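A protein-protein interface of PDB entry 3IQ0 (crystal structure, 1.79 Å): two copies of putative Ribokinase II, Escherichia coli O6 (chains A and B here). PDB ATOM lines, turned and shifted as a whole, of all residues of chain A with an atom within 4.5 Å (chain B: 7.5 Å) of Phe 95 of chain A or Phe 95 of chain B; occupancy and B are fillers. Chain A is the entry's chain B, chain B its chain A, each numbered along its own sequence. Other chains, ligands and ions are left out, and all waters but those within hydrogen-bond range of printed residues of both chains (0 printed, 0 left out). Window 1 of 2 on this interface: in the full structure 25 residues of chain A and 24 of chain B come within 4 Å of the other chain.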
ATOM      1  N   ILE A  16     -22.555 -23.712  26.165  1.00  0.00           N
ATOM      2  CA  ILE A  16     -21.641 -23.531  27.296  1.00  0.00           C
ATOM      3  C   ILE A  16     -21.951 -22.121  27.790  1.00  0.00           C
ATOM      4  O   ILE A  16     -21.718 -21.149  27.079  1.00  0.00           O
ATOM      5  CB  ILE A  16     -20.156 -23.618  26.870  1.00  0.00           C
ATOM      6  CG1 ILE A  16     -19.801 -25.047  26.444  1.00  0.00           C
ATOM      7  CG2 ILE A  16     -19.261 -23.204  28.026  1.00  0.00           C
ATOM      8  CD1 ILE A  16     -20.395 -25.471  25.133  1.00  0.00           C
ATOM      9  N   PHE A  25     -16.031 -12.706  26.880  1.00  0.00           N
ATOM     10  CA  PHE A  25     -15.507 -13.860  26.158  1.00  0.00           C
ATOM     11  C   PHE A  25     -13.984 -13.765  26.061  1.00  0.00           C
ATOM     12  O   PHE A  25     -13.310 -14.768  25.837  1.00  0.00           O
ATOM     13  CB  PHE A  25     -16.041 -13.898  24.720  1.00  0.00           C
ATOM     14  CG  PHE A  25     -17.484 -14.287  24.598  1.00  0.00           C
ATOM     15  CD1 PHE A  25     -17.923 -15.533  25.033  1.00  0.00           C
ATOM     16  CD2 PHE A  25     -18.396 -13.422  24.005  1.00  0.00           C
ATOM     17  CE1 PHE A  25     -19.246 -15.910  24.876  1.00  0.00           C
ATOM     18  CE2 PHE A  25     -19.716 -13.786  23.842  1.00  0.00           C
ATOM     19  CZ  PHE A  25     -20.148 -15.034  24.278  1.00  0.00           C
ATOM     20  N   TRP A  31     -17.192 -21.345  33.254  1.00  0.00           N
ATOM     21  CA  TRP A  31     -18.315 -21.604  32.362  1.00  0.00           C
ATOM     22  C   TRP A  31     -19.040 -22.867  32.804  1.00  0.00           C
ATOM     23  O   TRP A  31     -18.445 -23.743  33.425  1.00  0.00           O
ATOM     24  CB  TRP A  31     -17.830 -21.768  30.913  1.00  0.00           C
ATOM     25  CG  TRP A  31     -17.104 -20.568  30.391  1.00  0.00           C
ATOM     26  CD1 TRP A  31     -15.829 -20.181  30.700  1.00  0.00           C
ATOM     27  CD2 TRP A  31     -17.636 -19.550  29.533  1.00  0.00           C
ATOM     28  NE1 TRP A  31     -15.538 -18.983  30.092  1.00  0.00           N
ATOM     29  CE2 TRP A  31     -16.628 -18.572  29.371  1.00  0.00           C
ATOM     30  CE3 TRP A  31     -18.869 -19.368  28.889  1.00  0.00           C
ATOM     31  CZ2 TRP A  31     -16.815 -17.427  28.590  1.00  0.00           C
ATOM     32  CZ3 TRP A  31     -19.053 -18.224  28.111  1.00  0.00           C
ATOM     33  CH2 TRP A  31     -18.030 -17.271  27.972  1.00  0.00           C
ATOM     34  N   PHE A  65     -19.846 -34.174  23.125  1.00  0.00           N
ATOM     35  CA  PHE A  65     -20.856 -33.132  23.001  1.00  0.00           C
ATOM     36  C   PHE A  65     -21.982 -33.686  22.145  1.00  0.00           C
ATOM     37  O   PHE A  65     -23.147 -33.330  22.316  1.00  0.00           O
ATOM     38  CB  PHE A  65     -20.264 -31.880  22.353  1.00  0.00           C
ATOM     39  CG  PHE A  65     -19.332 -31.113  23.249  1.00  0.00           C
ATOM     40  CD1 PHE A  65     -19.246 -31.406  24.610  1.00  0.00           C
ATOM     41  CD2 PHE A  65     -18.577 -30.062  22.747  1.00  0.00           C
ATOM     42  CE1 PHE A  65     -18.428 -30.661  25.454  1.00  0.00           C
ATOM     43  CE2 PHE A  65     -17.755 -29.311  23.585  1.00  0.00           C
ATOM     44  CZ  PHE A  65     -17.681 -29.608  24.935  1.00  0.00           C
ATOM     45  N   SER A  93     -21.711 -25.978  18.618  1.00  0.00           N
ATOM     46  CA  SER A  93     -21.670 -25.450  19.973  1.00  0.00           C
ATOM     47  C   SER A  93     -22.036 -23.978  19.996  1.00  0.00           C
ATOM     48  O   SER A  93     -22.070 -23.311  18.957  1.00  0.00           O
ATOM     49  CB  SER A  93     -20.273 -25.610  20.561  1.00  0.00           C
ATOM     50  OG  SER A  93     -19.368 -24.719  19.926  1.00  0.00           O
ATOM     51  N   ALA A  94     -22.310 -23.476  21.192  1.00  0.00           N
ATOM     52  CA  ALA A  94     -22.654 -22.077  21.373  1.00  0.00           C
ATOM     53  C   ALA A  94     -22.245 -21.617  22.770  1.00  0.00           C
ATOM     54  O   ALA A  94     -22.649 -22.215  23.763  1.00  0.00           O
ATOM     55  CB  ALA A  94     -24.148 -21.875  21.181  1.00  0.00           C
ATOM     56  N   PHE A  95     -21.418 -20.577  22.828  1.00  0.00           N
ATOM     57  CA  PHE A  95     -20.977 -19.992  24.089  1.00  0.00           C
ATOM     58  C   PHE A  95     -21.870 -18.766  24.263  1.00  0.00           C
ATOM     59  O   PHE A  95     -22.054 -18.003  23.324  1.00  0.00           O
ATOM     60  CB  PHE A  95     -19.515 -19.535  24.003  1.00  0.00           C
ATOM     61  CG  PHE A  95     -18.518 -20.657  23.995  1.00  0.00           C
ATOM     62  CD1 PHE A  95     -17.954 -21.112  25.185  1.00  0.00           C
ATOM     63  CD2 PHE A  95     -18.124 -21.244  22.797  1.00  0.00           C
ATOM     64  CE1 PHE A  95     -17.010 -22.132  25.182  1.00  0.00           C
ATOM     65  CE2 PHE A  95     -17.178 -22.268  22.777  1.00  0.00           C
ATOM     66  CZ  PHE A  95     -16.620 -22.711  23.976  1.00  0.00           C
ATOM     67  N   VAL A  96     -22.417 -18.575  25.454  1.00  0.00           N
ATOM     68  CA  VAL A  96     -23.299 -17.441  25.692  1.00  0.00           C
ATOM     69  C   VAL A  96     -22.964 -16.723  27.003  1.00  0.00           C
ATOM     70  O   VAL A  96     -22.465 -17.333  27.946  1.00  0.00           O
ATOM     71  CB  VAL A  96     -24.787 -17.915  25.722  1.00  0.00           C
ATOM     72  CG1 VAL A  96     -24.978 -18.948  26.807  1.00  0.00           C
ATOM     73  CG2 VAL A  96     -25.715 -16.742  25.943  1.00  0.00           C
ATOM     74  N   ASP A 105     -25.619 -12.381  24.076  1.00  0.00           N
ATOM     75  CA  ASP A 105     -24.284 -12.454  23.460  1.00  0.00           C
ATOM     76  C   ASP A 105     -23.803 -13.883  23.217  1.00  0.00           C
ATOM     77  O   ASP A 105     -23.686 -14.684  24.147  1.00  0.00           O
ATOM     78  CB  ASP A 105     -23.260 -11.691  24.296  1.00  0.00           C
ATOM     79  CG  ASP A 105     -22.916 -10.346  23.692  1.00  0.00           C
ATOM     80  OD1 ASP A 105     -23.835  -9.514  23.520  1.00  0.00           O
ATOM     81  OD2 ASP A 105     -21.725 -10.122  23.382  1.00  0.00           O
ATOM     82  N   PHE A 106     -23.501 -14.192  21.957  1.00  0.00           N
ATOM     83  CA  PHE A 106     -23.083 -15.542  21.581  1.00  0.00           C
ATOM     84  C   PHE A 106     -21.837 -15.662  20.703  1.00  0.00           C
ATOM     85  O   PHE A 106     -21.427 -14.719  20.036  1.00  0.00           O
ATOM     86  CB  PHE A 106     -24.207 -16.231  20.800  1.00  0.00           C
ATOM     87  CG  PHE A 106     -25.485 -16.416  21.568  1.00  0.00           C
ATOM     88  CD1 PHE A 106     -25.732 -17.601  22.256  1.00  0.00           C
ATOM     89  CD2 PHE A 106     -26.466 -15.430  21.555  1.00  0.00           C
ATOM     90  CE1 PHE A 106     -26.941 -17.802  22.914  1.00  0.00           C
ATOM     91  CE2 PHE A 106     -27.678 -15.621  22.211  1.00  0.00           C
ATOM     92  CZ  PHE A 106     -27.917 -16.809  22.892  1.00  0.00           C
ATOM     93  N   ILE A 107     -21.258 -16.856  20.717  1.00  0.00           N
ATOM     94  CA  ILE A 107     -20.142 -17.215  19.847  1.00  0.00           C
ATOM     95  C   ILE A 107     -20.594 -18.567  19.322  1.00  0.00           C
ATOM     96  O   ILE A 107     -20.491 -19.582  20.014  1.00  0.00           O
ATOM     97  CB  ILE A 107     -18.793 -17.376  20.574  1.00  0.00           C
ATOM     98  CG1 ILE A 107     -18.227 -15.996  20.942  1.00  0.00           C
ATOM     99  CG2 ILE A 107     -17.810 -18.114  19.665  1.00  0.00           C
ATOM    100  CD1 ILE A 107     -16.838 -16.034  21.569  1.00  0.00           C
ATOM    101  N   LEU B  13      -5.750 -20.580  18.950  1.00  0.00           N
ATOM    102  CA  LEU B  13      -7.059 -20.954  19.460  1.00  0.00           C
ATOM    103  C   LEU B  13      -7.136 -20.704  20.946  1.00  0.00           C
ATOM    104  O   LEU B  13      -6.172 -20.262  21.568  1.00  0.00           O
ATOM    105  CB  LEU B  13      -7.333 -22.443  19.190  1.00  0.00           C
ATOM    106  CG  LEU B  13      -6.310 -23.474  19.692  1.00  0.00           C
ATOM    107  CD1 LEU B  13      -6.998 -24.761  20.109  1.00  0.00           C
ATOM    108  CD2 LEU B  13      -5.313 -23.752  18.601  1.00  0.00           C
ATOM    109  N   VAL B  14      -8.303 -20.966  21.514  1.00  0.00           N
ATOM    110  CA  VAL B  14      -8.469 -20.801  22.937  1.00  0.00           C
ATOM    111  C   VAL B  14      -8.710 -22.194  23.483  1.00  0.00           C
ATOM    112  O   VAL B  14      -9.273 -23.056  22.792  1.00  0.00           O
ATOM    113  CB  VAL B  14      -9.674 -19.891  23.285  1.00  0.00           C
ATOM    114  CG1 VAL B  14      -9.461 -18.500  22.691  1.00  0.00           C
ATOM    115  CG2 VAL B  14     -10.966 -20.508  22.776  1.00  0.00           C
ATOM    116  N   GLU B  15      -8.249 -22.424  24.703  1.00  0.00           N
ATOM    117  CA  GLU B  15      -8.450 -23.705  25.339  1.00  0.00           C
ATOM    118  C   GLU B  15      -9.416 -23.500  26.502  1.00  0.00           C
ATOM    119  O   GLU B  15      -9.371 -22.477  27.189  1.00  0.00           O
ATOM    120  CB  GLU B  15      -7.126 -24.274  25.853  1.00  0.00           C
ATOM    121  CG  GLU B  15      -7.125 -25.796  25.899  1.00  0.00           C
ATOM    122  CD  GLU B  15      -5.846 -26.377  26.465  1.00  0.00           C
ATOM    123  OE1 GLU B  15      -5.616 -26.228  27.679  1.00  0.00           O
ATOM    124  OE2 GLU B  15      -5.073 -26.983  25.694  1.00  0.00           O
ATOM    125  N   ILE B  16     -10.300 -24.474  26.684  1.00  0.00           N
ATOM    126  CA  ILE B  16     -11.302 -24.486  27.751  1.00  0.00           C
ATOM    127  C   ILE B  16     -10.948 -25.745  28.534  1.00  0.00           C
ATOM    128  O   ILE B  16     -11.009 -26.845  27.985  1.00  0.00           O
ATOM    129  CB  ILE B  16     -12.717 -24.633  27.160  1.00  0.00           C
ATOM    130  CG1 ILE B  16     -12.980 -23.500  26.157  1.00  0.00           C
ATOM    131  CG2 ILE B  16     -13.757 -24.631  28.276  1.00  0.00           C
ATOM    132  CD1 ILE B  16     -13.081 -22.118  26.793  1.00  0.00           C
ATOM    133  N   MET B  17     -10.568 -25.593  29.801  1.00  0.00           N
ATOM    134  CA  MET B  17     -10.150 -26.739  30.613  1.00  0.00           C
ATOM    135  C   MET B  17     -11.161 -27.209  31.659  1.00  0.00           C
ATOM    136  O   MET B  17     -11.745 -26.399  32.372  1.00  0.00           O
ATOM    137  CB  MET B  17      -8.827 -26.399  31.315  1.00  0.00           C
ATOM    138  CG  MET B  17      -7.764 -25.824  30.389  1.00  0.00           C
ATOM    139  SD  MET B  17      -6.188 -25.167  31.340  1.00  0.00           S
ATOM    140  CE  MET B  17      -5.372 -26.881  31.638  1.00  0.00           C
ATOM    141  N   ALA B  18     -11.350 -28.522  31.760  1.00  0.00           N
ATOM    142  CA  ALA B  18     -12.280 -29.070  32.742  1.00  0.00           C
ATOM    143  C   ALA B  18     -11.770 -28.700  34.126  1.00  0.00           C
ATOM    144  O   ALA B  18     -10.557 -28.608  34.345  1.00  0.00           O
ATOM    145  CB  ALA B  18     -12.378 -30.585  32.603  1.00  0.00           C
ATOM    146  N   PHE B  25     -16.919 -35.323  28.987  1.00  0.00           N
ATOM    147  CA  PHE B  25     -17.353 -34.344  28.002  1.00  0.00           C
ATOM    148  C   PHE B  25     -18.880 -34.393  27.871  1.00  0.00           C
ATOM    149  O   PHE B  25     -19.511 -33.392  27.540  1.00  0.00           O
ATOM    150  CB  PHE B  25     -16.726 -34.642  26.631  1.00  0.00           C
ATOM    151  CG  PHE B  25     -15.299 -34.172  26.488  1.00  0.00           C
ATOM    152  CD1 PHE B  25     -14.963 -32.838  26.717  1.00  0.00           C
ATOM    153  CD2 PHE B  25     -14.302 -35.048  26.084  1.00  0.00           C
ATOM    154  CE1 PHE B  25     -13.655 -32.386  26.546  1.00  0.00           C
ATOM    155  CE2 PHE B  25     -12.982 -34.603  25.907  1.00  0.00           C
ATOM    156  CZ  PHE B  25     -12.663 -33.270  26.138  1.00  0.00           C
ATOM    157  N   TRP B  31     -16.106 -25.488  33.736  1.00  0.00           N
ATOM    158  CA  TRP B  31     -14.915 -25.346  32.909  1.00  0.00           C
ATOM    159  C   TRP B  31     -14.237 -24.008  33.153  1.00  0.00           C
ATOM    160  O   TRP B  31     -14.876 -23.042  33.568  1.00  0.00           O
ATOM    161  CB  TRP B  31     -15.274 -25.462  31.421  1.00  0.00           C
ATOM    162  CG  TRP B  31     -15.947 -26.746  31.056  1.00  0.00           C
ATOM    163  CD1 TRP B  31     -17.257 -27.074  31.248  1.00  0.00           C
ATOM    164  CD2 TRP B  31     -15.323 -27.901  30.492  1.00  0.00           C
ATOM    165  NE1 TRP B  31     -17.489 -28.367  30.841  1.00  0.00           N
ATOM    166  CE2 TRP B  31     -16.317 -28.898  30.373  1.00  0.00           C
ATOM    167  CE3 TRP B  31     -14.018 -28.194  30.079  1.00  0.00           C
ATOM    168  CZ2 TRP B  31     -16.044 -30.167  29.861  1.00  0.00           C
ATOM    169  CZ3 TRP B  31     -13.747 -29.455  29.571  1.00  0.00           C
ATOM    170  CH2 TRP B  31     -14.755 -30.426  29.466  1.00  0.00           C
ATOM    171  N   GLY B  33     -11.624 -20.994  31.493  1.00  0.00           N
ATOM    172  CA  GLY B  33     -11.116 -20.477  30.238  1.00  0.00           C
ATOM    173  C   GLY B  33     -11.932 -19.287  29.788  1.00  0.00           C
ATOM    174  O   GLY B  33     -12.754 -18.776  30.552  1.00  0.00           O
ATOM    175  N   PRO B  34     -11.726 -18.815  28.551  1.00  0.00           N
ATOM    176  CA  PRO B  34     -10.756 -19.385  27.611  1.00  0.00           C
ATOM    177  C   PRO B  34      -9.323 -18.977  27.958  1.00  0.00           C
ATOM    178  O   PRO B  34      -9.110 -17.978  28.643  1.00  0.00           O
ATOM    179  CB  PRO B  34     -11.199 -18.791  26.286  1.00  0.00           C
ATOM    180  CG  PRO B  34     -11.585 -17.384  26.705  1.00  0.00           C
ATOM    181  CD  PRO B  34     -12.406 -17.645  27.961  1.00  0.00           C
ATOM    182  N   PHE B  65     -12.884 -14.686  21.558  1.00  0.00           N
ATOM    183  CA  PHE B  65     -11.862 -15.720  21.624  1.00  0.00           C
ATOM    184  C   PHE B  65     -10.649 -15.325  20.794  1.00  0.00           C
ATOM    185  O   PHE B  65      -9.513 -15.660  21.139  1.00  0.00           O
ATOM    186  CB  PHE B  65     -12.426 -17.067  21.153  1.00  0.00           C
ATOM    187  CG  PHE B  65     -13.337 -17.725  22.157  1.00  0.00           C
ATOM    188  CD1 PHE B  65     -13.451 -17.219  23.452  1.00  0.00           C
ATOM    189  CD2 PHE B  65     -14.059 -18.860  21.821  1.00  0.00           C
ATOM    190  CE1 PHE B  65     -14.273 -17.836  24.399  1.00  0.00           C
ATOM    191  CE2 PHE B  65     -14.885 -19.490  22.758  1.00  0.00           C
ATOM    192  CZ  PHE B  65     -14.994 -18.977  24.050  1.00  0.00           C
ATOM    193  N   THR B  91     -13.313 -18.346  15.973  1.00  0.00           N
ATOM    194  CA  THR B  91     -11.947 -18.613  16.402  1.00  0.00           C
ATOM    195  C   THR B  91     -11.889 -20.067  16.873  1.00  0.00           C
ATOM    196  O   THR B  91     -12.828 -20.558  17.499  1.00  0.00           O
ATOM    197  CB  THR B  91     -11.567 -17.671  17.550  1.00  0.00           C
ATOM    198  OG1 THR B  91     -11.602 -16.322  17.069  1.00  0.00           O
ATOM    199  CG2 THR B  91     -10.180 -17.997  18.098  1.00  0.00           C
ATOM    200  N   SER B  93     -11.056 -23.550  18.848  1.00  0.00           N
ATOM    201  CA  SER B  93     -11.136 -23.862  20.268  1.00  0.00           C
ATOM    202  C   SER B  93     -10.786 -25.312  20.534  1.00  0.00           C
ATOM    203  O   SER B  93     -10.783 -26.152  19.625  1.00  0.00           O
ATOM    204  CB  SER B  93     -12.553 -23.614  20.771  1.00  0.00           C
ATOM    205  OG  SER B  93     -13.445 -24.545  20.179  1.00  0.00           O
ATOM    206  N   ALA B  94     -10.500 -25.601  21.798  1.00  0.00           N
ATOM    207  CA  ALA B  94     -10.181 -26.956  22.216  1.00  0.00           C
ATOM    208  C   ALA B  94     -10.604 -27.157  23.662  1.00  0.00           C
ATOM    209  O   ALA B  94     -10.200 -26.408  24.550  1.00  0.00           O
ATOM    210  CB  ALA B  94      -8.686 -27.228  22.057  1.00  0.00           C
ATOM    211  N   PHE B  95     -11.454 -28.153  23.881  1.00  0.00           N
ATOM    212  CA  PHE B  95     -11.914 -28.502  25.220  1.00  0.00           C
ATOM    213  C   PHE B  95     -11.019 -29.653  25.651  1.00  0.00           C
ATOM    214  O   PHE B  95     -10.824 -30.596  24.889  1.00  0.00           O
ATOM    215  CB  PHE B  95     -13.359 -29.000  25.186  1.00  0.00           C
ATOM    216  CG  PHE B  95     -14.381 -27.912  25.014  1.00  0.00           C
ATOM    217  CD1 PHE B  95     -15.068 -27.404  26.116  1.00  0.00           C
ATOM    218  CD2 PHE B  95     -14.672 -27.413  23.753  1.00  0.00           C
ATOM    219  CE1 PHE B  95     -16.035 -26.414  25.958  1.00  0.00           C
ATOM    220  CE2 PHE B  95     -15.637 -26.423  23.584  1.00  0.00           C
ATOM    221  CZ  PHE B  95     -16.318 -25.926  24.688  1.00  0.00           C
ATOM    222  N   VAL B  96     -10.476 -29.587  26.859  1.00  0.00           N
ATOM    223  CA  VAL B  96      -9.611 -30.656  27.334  1.00  0.00           C
ATOM    224  C   VAL B  96      -9.995 -31.127  28.725  1.00  0.00           C
ATOM    225  O   VAL B  96     -10.361 -30.333  29.581  1.00  0.00           O
ATOM    226  CB  VAL B  96      -8.127 -30.219  27.353  1.00  0.00           C
ATOM    227  CG1 VAL B  96      -7.957 -28.971  28.200  1.00  0.00           C
ATOM    228  CG2 VAL B  96      -7.254 -31.350  27.883  1.00  0.00           C
ATOM    229  N   THR B  97      -9.928 -32.436  28.926  1.00  0.00           N
ATOM    230  CA  THR B  97     -10.235 -33.023  30.217  1.00  0.00           C
ATOM    231  C   THR B  97      -9.090 -33.948  30.615  1.00  0.00           C
ATOM    232  O   THR B  97      -8.367 -34.459  29.757  1.00  0.00           O
ATOM    233  CB  THR B  97     -11.538 -33.824  30.187  1.00  0.00           C
ATOM    234  OG1 THR B  97     -11.770 -34.374  31.489  1.00  0.00           O
ATOM    235  CG2 THR B  97     -11.451 -34.957  29.165  1.00  0.00           C
ATOM    236  N   ASP B 105      -7.604 -35.795  27.009  1.00  0.00           N
ATOM    237  CA  ASP B 105      -8.690 -35.996  26.052  1.00  0.00           C
ATOM    238  C   ASP B 105      -9.102 -34.629  25.530  1.00  0.00           C
ATOM    239  O   ASP B 105      -9.123 -33.660  26.284  1.00  0.00           O
ATOM    240  CB  ASP B 105      -9.872 -36.694  26.713  1.00  0.00           C
ATOM    241  CG  ASP B 105      -9.918 -38.175  26.402  1.00  0.00           C
ATOM    242  OD1 ASP B 105      -8.868 -38.847  26.501  1.00  0.00           O
ATOM    243  OD2 ASP B 105     -11.013 -38.672  26.065  1.00  0.00           O
ATOM    244  N   PHE B 106      -9.438 -34.552  24.247  1.00  0.00           N
ATOM    245  CA  PHE B 106      -9.792 -33.274  23.639  1.00  0.00           C
ATOM    246  C   PHE B 106     -10.969 -33.316  22.675  1.00  0.00           C
ATOM    247  O   PHE B 106     -11.293 -34.354  22.113  1.00  0.00           O
ATOM    248  CB  PHE B 106      -8.613 -32.732  22.814  1.00  0.00           C
ATOM    249  CG  PHE B 106      -7.344 -32.504  23.590  1.00  0.00           C
ATOM    250  CD1 PHE B 106      -6.996 -31.223  24.010  1.00  0.00           C
ATOM    251  CD2 PHE B 106      -6.457 -33.550  23.823  1.00  0.00           C
ATOM    252  CE1 PHE B 106      -5.771 -30.980  24.646  1.00  0.00           C
ATOM    253  CE2 PHE B 106      -5.230 -33.321  24.458  1.00  0.00           C
ATOM    254  CZ  PHE B 106      -4.887 -32.034  24.868  1.00  0.00           C
ATOM    255  N   ILE B 107     -11.577 -32.151  22.477  1.00  0.00           N
ATOM    256  CA  ILE B 107     -12.644 -31.967  21.495  1.00  0.00           C
ATOM    257  C   ILE B 107     -12.130 -30.737  20.762  1.00  0.00           C
ATOM    258  O   ILE B 107     -12.111 -29.640  21.312  1.00  0.00           O
ATOM    259  CB  ILE B 107     -14.023 -31.663  22.127  1.00  0.00           C
ATOM    260  CG1 ILE B 107     -14.603 -32.951  22.737  1.00  0.00           C
ATOM    261  CG2 ILE B 107     -14.969 -31.112  21.063  1.00  0.00           C
ATOM    262  CD1 ILE B 107     -16.041 -32.832  23.227  1.00  0.00           C
ATOM    263  N   PHE B 108     -11.682 -30.938  19.529  1.00  0.00           N
ATOM    264  CA  PHE B 108     -11.105 -29.864  18.734  1.00  0.00           C
ATOM    265  C   PHE B 108     -11.993 -29.246  17.684  1.00  0.00           C
ATOM    266  O   PHE B 108     -12.768 -29.933  17.024  1.00  0.00           O
ATOM    267  CB  PHE B 108      -9.871 -30.361  17.974  1.00  0.00           C
ATOM    268  CG  PHE B 108      -8.694 -30.683  18.835  1.00  0.00           C
ATOM    269  CD1 PHE B 108      -8.024 -29.678  19.532  1.00  0.00           C
ATOM    270  CD2 PHE B 108      -8.224 -31.991  18.919  1.00  0.00           C
ATOM    271  CE1 PHE B 108      -6.903 -29.970  20.294  1.00  0.00           C
ATOM    272  CE2 PHE B 108      -7.101 -32.296  19.682  1.00  0.00           C
ATOM    273  CZ  PHE B 108      -6.438 -31.283  20.371  1.00  0.00           C
ATOM    274  N   ASN B 109     -11.860 -27.934  17.543  1.00  0.00           N
ATOM    275  CA  ASN B 109     -12.516 -27.212  16.473  1.00  0.00           C
ATOM    276  C   ASN B 109     -11.394 -26.345  15.919  1.00  0.00           C
ATOM    277  O   ASN B 109     -11.273 -25.163  16.251  1.00  0.00           O
ATOM    278  CB  ASN B 109     -13.669 -26.319  16.909  1.00  0.00           C
ATOM    279  CG  ASN B 109     -14.309 -25.628  15.708  1.00  0.00           C
ATOM    280  OD1 ASN B 109     -14.374 -26.219  14.619  1.00  0.00           O
ATOM    281  ND2 ASN B 109     -14.767 -24.392  15.882  1.00  0.00           N
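N of Trp 31 of chain A sits at hydrogen-bond distance from O of Trp 31 of chain B. O of Gly 33 of chain B is in hydrogen-bond range of NE1 of Trp 31 of chain A.
The backbone carbonyl oxygen (O) of Phe 95 of chain B lies within hydrogen-bond range of the backbone NH (N) of Ile 107 of chain B (3.0 Å). N of Ile 16 of chain A lies within hydrogen-bond range of O of Ala 94 of chain A (2.8 Å). N of Val 96 of chain A lies within hydrogen-bond range of O of Ile 16 of chain A. The backbone carbonyl oxygen (O) of Phe 95 of chain A lies within hydrogen-bond range of the backbone NH (N) of Ile 107 of chain A (3.0 Å).
Among the printed residues, pairs that only touch across the chains: Phe 25 of chain A with Pro 34 of chain B (3.3 Å), Phe 95 of chain A with Phe 95 of chain B (3.3 Å), Phe 25 of chain A with Phe 65 of chain B (3.4 Å), Phe 65 of chain A with Phe 25 of chain B (3.5 Å), Phe 65 of chain A with Phe 95 of chain B (3.6 Å), Phe 95 of chain A with Phe 65 of chain B (3.6 Å), Phe 65 of chain A with Ile 107 of chain B (3.7 Å), Ile 107 of chain A with Phe 65 of chain B (3.9 Å) and Ile 16 of chain A with Phe 95 of chain B (3.998 Å).
Phe 95 of chain A touches just these residues of chain B: Phe 65 and Phe 95. Printed residues of chain A within 4 Å of Phe 95 of chain B: Ile 16 (3.998 Å), Phe 65 (3.6 Å) and Phe 95 (3.3 Å). No residue of chain B comes within 4 Å of Ala 94 of chain A. Printed residues of chain A within 4 Å of Trp 31 of chain B: Trp 31. Of the printed residues of chain B, Ile 107 of chain A touches Phe 65. Met 17 of chain B touches none of the printed residues of chain A. The nearest residue of chain B that does not touch Phe 95 of chain A is Ile 16 of chain B (4.2 Å).
Of the 22 printed residues of chain B, 7 touch a printed residue of chain A. Hydrophobic or aromatic side chains of chain B that line the printed part of chain A: Pro 34, Phe 65, Phe 95 and Ile 107. Of the 11 printed residues of chain A, 6 touch a printed residue of chain B. Hydrophobic or aromatic side chains of chain A that line the printed part of chain B: Ile 16, Trp 31, Phe 65, Phe 95 and Ile 107.
Phe 25 of chain A touches Phe 65 of chain B, and with the chains exchanged Phe 65 of chain A touches Phe 25 of chain B. Trp 31 of chain B touches its own counterpart, Trp 31 of chain A. Phe 65 of chain A touches Phe 95 of chain B, and with the chains exchanged Phe 95 of chain A touches Phe 65 of chain B. Phe 95 of chain B touches its own counterpart, Phe 95 of chain A. Positions printed for both chains: 16, 25, 31, 65, 93, 94, 95, 96, 105, 106 and 107.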
